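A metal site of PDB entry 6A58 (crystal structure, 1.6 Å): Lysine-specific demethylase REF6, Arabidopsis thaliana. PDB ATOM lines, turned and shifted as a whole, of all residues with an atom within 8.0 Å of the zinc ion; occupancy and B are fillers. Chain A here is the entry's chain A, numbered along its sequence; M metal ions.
A ring nitrogen (NE2) of His 100 binds the zinc ion (2.1 Å). A ring nitrogen (NE2) of His 96 is bound to the zinc ion (2.1 Å). SG of Cys 78 is bound to the zinc ion (2.3 Å). SG of Cys 83 binds the zinc ion, 2.3 Å away.
The backbone NH (N) of Trp 80 lies close to the side-chain sulfur (SG) of Cys 78, 3.5 Å away. The backbone NH (N) of Cys 78 lies within hydrogen-bond range of the backbone carbonyl oxygen (O) of Met 85. The backbone NH of Met 85 sits close to the side-chain sulfur of Cys 83 (3.6 Å).
Four residues have an atom within 4 Å of the zinc ion: Cys 78, Cys 83, His 96 and His 100. The nearest printed residue that does not touch the zinc ion is Trp 80 (4.2 Å).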
ATOM      1  N   LYS A  77      13.575   8.060  -7.448  1.00  0.00           N
ATOM      2  CA  LYS A  77      12.675   7.520  -8.473  1.00  0.00           C
ATOM      3  C   LYS A  77      13.282   7.689  -9.854  1.00  0.00           C
ATOM      4  O   LYS A  77      13.944   8.681 -10.129  1.00  0.00           O
ATOM      5  CB  LYS A  77      11.321   8.242  -8.446  1.00  0.00           C
ATOM      6  CG  LYS A  77      10.467   7.944  -7.217  1.00  0.00           C
ATOM      7  CD  LYS A  77       9.074   8.542  -7.354  1.00  0.00           C
ATOM      8  CE  LYS A  77       8.105   7.951  -6.338  1.00  0.00           C
ATOM      9  NZ  LYS A  77       8.495   8.258  -4.937  1.00  0.00           N
ATOM     10  N   CYS A  78      13.041   6.715 -10.721  1.00  0.00           N
ATOM     11  CA  CYS A  78      13.434   6.833 -12.122  1.00  0.00           C
ATOM     12  C   CYS A  78      12.640   7.975 -12.760  1.00  0.00           C
ATOM     13  O   CYS A  78      11.428   8.064 -12.572  1.00  0.00           O
ATOM     14  CB  CYS A  78      13.161   5.533 -12.866  1.00  0.00           C
ATOM     15  SG  CYS A  78      13.667   5.611 -14.603  1.00  0.00           S
ATOM     16  N   PRO A  79      13.319   8.858 -13.523  1.00  0.00           N
ATOM     17  CA  PRO A  79      12.634   9.984 -14.151  1.00  0.00           C
ATOM     18  C   PRO A  79      11.926   9.655 -15.469  1.00  0.00           C
ATOM     19  O   PRO A  79      11.260  10.531 -16.019  1.00  0.00           O
ATOM     20  CB  PRO A  79      13.776  10.965 -14.416  1.00  0.00           C
ATOM     21  CG  PRO A  79      14.940  10.091 -14.687  1.00  0.00           C
ATOM     22  CD  PRO A  79      14.780   8.921 -13.746  1.00  0.00           C
ATOM     23  N   TRP A  80      12.051   8.417 -15.959  1.00  0.00           N
ATOM     24  CA  TRP A  80      11.469   8.017 -17.247  1.00  0.00           C
ATOM     25  C   TRP A  80       9.978   7.738 -17.066  1.00  0.00           C
ATOM     26  O   TRP A  80       9.613   6.831 -16.311  1.00  0.00           O
ATOM     27  CB  TRP A  80      12.187   6.749 -17.758  1.00  0.00           C
ATOM     28  CG  TRP A  80      12.248   6.580 -19.248  1.00  0.00           C
ATOM     29  CD1 TRP A  80      11.547   5.690 -19.994  1.00  0.00           C
ATOM     30  CD2 TRP A  80      13.106   7.284 -20.146  1.00  0.00           C
ATOM     31  NE1 TRP A  80      11.901   5.803 -21.320  1.00  0.00           N
ATOM     32  CE2 TRP A  80      12.841   6.785 -21.444  1.00  0.00           C
ATOM     33  CE3 TRP A  80      14.055   8.309 -19.996  1.00  0.00           C
ATOM     34  CZ2 TRP A  80      13.517   7.267 -22.581  1.00  0.00           C
ATOM     35  CZ3 TRP A  80      14.720   8.778 -21.119  1.00  0.00           C
ATOM     36  CH2 TRP A  80      14.439   8.255 -22.394  1.00  0.00           C
ATOM     37  N   LYS A  81       9.116   8.505 -17.737  1.00  0.00           N
ATOM     38  CA  LYS A  81       7.664   8.318 -17.610  1.00  0.00           C
ATOM     39  C   LYS A  81       7.280   6.872 -17.895  1.00  0.00           C
ATOM     40  O   LYS A  81       7.785   6.271 -18.846  1.00  0.00           O
ATOM     41  CB  LYS A  81       6.905   9.248 -18.563  1.00  0.00           C
ATOM     42  CG  LYS A  81       6.968  10.725 -18.198  1.00  0.00           C
ATOM     43  CD  LYS A  81       6.522  11.598 -19.363  1.00  0.00           C
ATOM     44  CE  LYS A  81       5.052  11.429 -19.702  1.00  0.00           C
ATOM     45  NZ  LYS A  81       4.638  12.272 -20.855  1.00  0.00           N
ATOM     46  N   GLY A  82       6.388   6.329 -17.069  1.00  0.00           N
ATOM     47  CA  GLY A  82       5.969   4.934 -17.155  1.00  0.00           C
ATOM     48  C   GLY A  82       6.751   3.949 -16.296  1.00  0.00           C
ATOM     49  O   GLY A  82       6.288   2.838 -16.060  1.00  0.00           O
ATOM     50  N   CYS A  83       7.943   4.355 -15.842  1.00  0.00           N
ATOM     51  CA  CYS A  83       8.800   3.493 -15.050  1.00  0.00           C
ATOM     52  C   CYS A  83       8.574   3.755 -13.567  1.00  0.00           C
ATOM     53  O   CYS A  83       8.602   4.900 -13.129  1.00  0.00           O
ATOM     54  CB  CYS A  83      10.266   3.737 -15.387  1.00  0.00           C
ATOM     55  SG  CYS A  83      11.377   2.565 -14.608  1.00  0.00           S
ATOM     56  N   LYS A  84       8.357   2.674 -12.815  1.00  0.00           N
ATOM     57  CA  LYS A  84       8.077   2.767 -11.371  1.00  0.00           C
ATOM     58  C   LYS A  84       9.265   2.315 -10.522  1.00  0.00           C
ATOM     59  O   LYS A  84       9.123   2.165  -9.305  1.00  0.00           O
ATOM     60  CB  LYS A  84       6.822   1.936 -11.043  1.00  0.00           C
ATOM     61  CG  LYS A  84       5.593   2.348 -11.842  1.00  0.00           C
ATOM     62  CD  LYS A  84       4.316   1.745 -11.284  1.00  0.00           C
ATOM     63  CE  LYS A  84       3.099   2.249 -12.047  1.00  0.00           C
ATOM     64  NZ  LYS A  84       1.813   1.842 -11.420  1.00  0.00           N
ATOM     65  N   MET A  85      10.428   2.124 -11.133  1.00  0.00           N
ATOM     66  CA  MET A  85      11.602   1.644 -10.411  1.00  0.00           C
ATOM     67  C   MET A  85      12.192   2.734  -9.525  1.00  0.00           C
ATOM     68  O   MET A  85      12.139   3.909  -9.858  1.00  0.00           O
ATOM     69  CB  MET A  85      12.674   1.111 -11.371  1.00  0.00           C
ATOM     70  CG  MET A  85      12.214  -0.116 -12.150  1.00  0.00           C
ATOM     71  SD  MET A  85      13.579  -1.139 -12.750  1.00  0.00           S
ATOM     72  CE  MET A  85      14.185  -1.836 -11.216  1.00  0.00           C
ATOM     73  N   THR A  86      12.731   2.301  -8.388  1.00  0.00           N
ATOM     74  CA  THR A  86      13.290   3.194  -7.375  1.00  0.00           C
ATOM     75  C   THR A  86      14.657   2.694  -6.942  1.00  0.00           C
ATOM     76  O   THR A  86      14.967   1.499  -7.100  1.00  0.00           O
ATOM     77  CB  THR A  86      12.359   3.283  -6.147  1.00  0.00           C
ATOM     78  OG1 THR A  86      12.057   1.965  -5.682  1.00  0.00           O
ATOM     79  CG2 THR A  86      11.082   4.013  -6.499  1.00  0.00           C
ATOM     80  N   PHE A  87      15.477   3.599  -6.422  1.00  0.00           N
ATOM     81  CA  PHE A  87      16.890   3.300  -6.129  1.00  0.00           C
ATOM     82  C   PHE A  87      17.370   3.912  -4.823  1.00  0.00           C
ATOM     83  O   PHE A  87      16.897   4.975  -4.412  1.00  0.00           O
ATOM     84  CB  PHE A  87      17.762   3.780  -7.293  1.00  0.00           C
ATOM     85  CG  PHE A  87      17.358   3.161  -8.592  1.00  0.00           C
ATOM     86  CD1 PHE A  87      17.818   1.901  -8.932  1.00  0.00           C
ATOM     87  CD2 PHE A  87      16.436   3.797  -9.421  1.00  0.00           C
ATOM     88  CE1 PHE A  87      17.404   1.293 -10.105  1.00  0.00           C
ATOM     89  CE2 PHE A  87      16.026   3.200 -10.602  1.00  0.00           C
ATOM     90  CZ  PHE A  87      16.514   1.949 -10.940  1.00  0.00           C
ATOM     91  N   ARG A  93      20.703   4.528 -10.036  1.00  0.00           N
ATOM     92  CA  ARG A  93      19.650   5.133 -10.851  1.00  0.00           C
ATOM     93  C   ARG A  93      20.202   5.572 -12.208  1.00  0.00           C
ATOM     94  O   ARG A  93      19.585   5.304 -13.232  1.00  0.00           O
ATOM     95  CB  ARG A  93      18.995   6.335 -10.152  1.00  0.00           C
ATOM     96  CG  ARG A  93      17.985   7.065 -11.023  1.00  0.00           C
ATOM     97  CD  ARG A  93      17.119   8.038 -10.238  1.00  0.00           C
ATOM     98  NE  ARG A  93      17.879   9.168  -9.712  1.00  0.00           N
ATOM     99  CZ  ARG A  93      17.354  10.216  -9.076  1.00  0.00           C
ATOM    100  NH1 ARG A  93      16.041  10.294  -8.866  1.00  0.00           N
ATOM    101  NH2 ARG A  93      18.147  11.189  -8.627  1.00  0.00           N
ATOM    102  N   HIS A  96      20.749   2.623 -14.392  1.00  0.00           N
ATOM    103  CA  HIS A  96      19.439   2.146 -14.843  1.00  0.00           C
ATOM    104  C   HIS A  96      18.841   2.960 -15.994  1.00  0.00           C
ATOM    105  O   HIS A  96      18.284   2.383 -16.925  1.00  0.00           O
ATOM    106  CB  HIS A  96      18.439   2.120 -13.689  1.00  0.00           C
ATOM    107  CG  HIS A  96      17.024   1.979 -14.139  1.00  0.00           C
ATOM    108  ND1 HIS A  96      16.491   0.778 -14.542  1.00  0.00           N
ATOM    109  CD2 HIS A  96      16.028   2.886 -14.277  1.00  0.00           C
ATOM    110  CE1 HIS A  96      15.228   0.951 -14.898  1.00  0.00           C
ATOM    111  NE2 HIS A  96      14.924   2.221 -14.746  1.00  0.00           N
ATOM    112  N   ILE A  97      18.963   4.286 -15.933  1.00  0.00           N
ATOM    113  CA  ILE A  97      18.397   5.165 -16.973  1.00  0.00           C
ATOM    114  C   ILE A  97      18.973   4.825 -18.366  1.00  0.00           C
ATOM    115  O   ILE A  97      18.277   4.967 -19.372  1.00  0.00           O
ATOM    116  CB  ILE A  97      18.590   6.660 -16.628  1.00  0.00           C
ATOM    117  CG1 ILE A  97      17.744   7.031 -15.402  1.00  0.00           C
ATOM    118  CG2 ILE A  97      18.178   7.566 -17.794  1.00  0.00           C
ATOM    119  CD1 ILE A  97      18.190   8.289 -14.691  1.00  0.00           C
ATOM    120  N   ARG A  98      20.218   4.341 -18.406  1.00  0.00           N
ATOM    121  CA  ARG A  98      20.825   3.909 -19.668  1.00  0.00           C
ATOM    122  C   ARG A  98      20.061   2.772 -20.350  1.00  0.00           C
ATOM    123  O   ARG A  98      20.124   2.643 -21.573  1.00  0.00           O
ATOM    124  CB  ARG A  98      22.287   3.499 -19.469  1.00  0.00           C
ATOM    125  CG  ARG A  98      23.198   4.630 -19.003  1.00  0.00           C
ATOM    126  CD  ARG A  98      24.563   4.102 -18.624  1.00  0.00           C
ATOM    127  NE  ARG A  98      25.316   5.105 -17.869  1.00  0.00           N
ATOM    128  CZ  ARG A  98      26.354   4.842 -17.075  1.00  0.00           C
ATOM    129  NH1 ARG A  98      26.800   3.589 -16.904  1.00  0.00           N
ATOM    130  NH2 ARG A  98      26.951   5.835 -16.430  1.00  0.00           N
ATOM    131  N   VAL A  99      19.332   1.970 -19.576  1.00  0.00           N
ATOM    132  CA  VAL A  99      18.470   0.908 -20.151  1.00  0.00           C
ATOM    133  C   VAL A  99      17.402   1.544 -21.034  1.00  0.00           C
ATOM    134  O   VAL A  99      17.109   1.027 -22.112  1.00  0.00           O
ATOM    135  CB  VAL A  99      17.817   0.027 -19.058  1.00  0.00           C
ATOM    136  CG1 VAL A  99      16.875  -1.012 -19.670  1.00  0.00           C
ATOM    137  CG2 VAL A  99      18.880  -0.656 -18.208  1.00  0.00           C
ATOM    138  N   HIS A 100      16.833   2.664 -20.578  1.00  0.00           N
ATOM    139  CA  HIS A 100      15.811   3.390 -21.343  1.00  0.00           C
ATOM    140  C   HIS A 100      16.386   4.140 -22.538  1.00  0.00           C
ATOM    141  O   HIS A 100      15.763   4.162 -23.600  1.00  0.00           O
ATOM    142  CB  HIS A 100      15.097   4.403 -20.456  1.00  0.00           C
ATOM    143  CG  HIS A 100      14.368   3.810 -19.300  1.00  0.00           C
ATOM    144  ND1 HIS A 100      13.467   2.772 -19.431  1.00  0.00           N
ATOM    145  CD2 HIS A 100      14.377   4.133 -17.980  1.00  0.00           C
ATOM    146  CE1 HIS A 100      12.977   2.462 -18.243  1.00  0.00           C
ATOM    147  NE2 HIS A 100      13.501   3.278 -17.348  1.00  0.00           N
HETATM  148 ZN    ZN M   1      13.331   3.482 -15.293  1.00  0.00          ZN
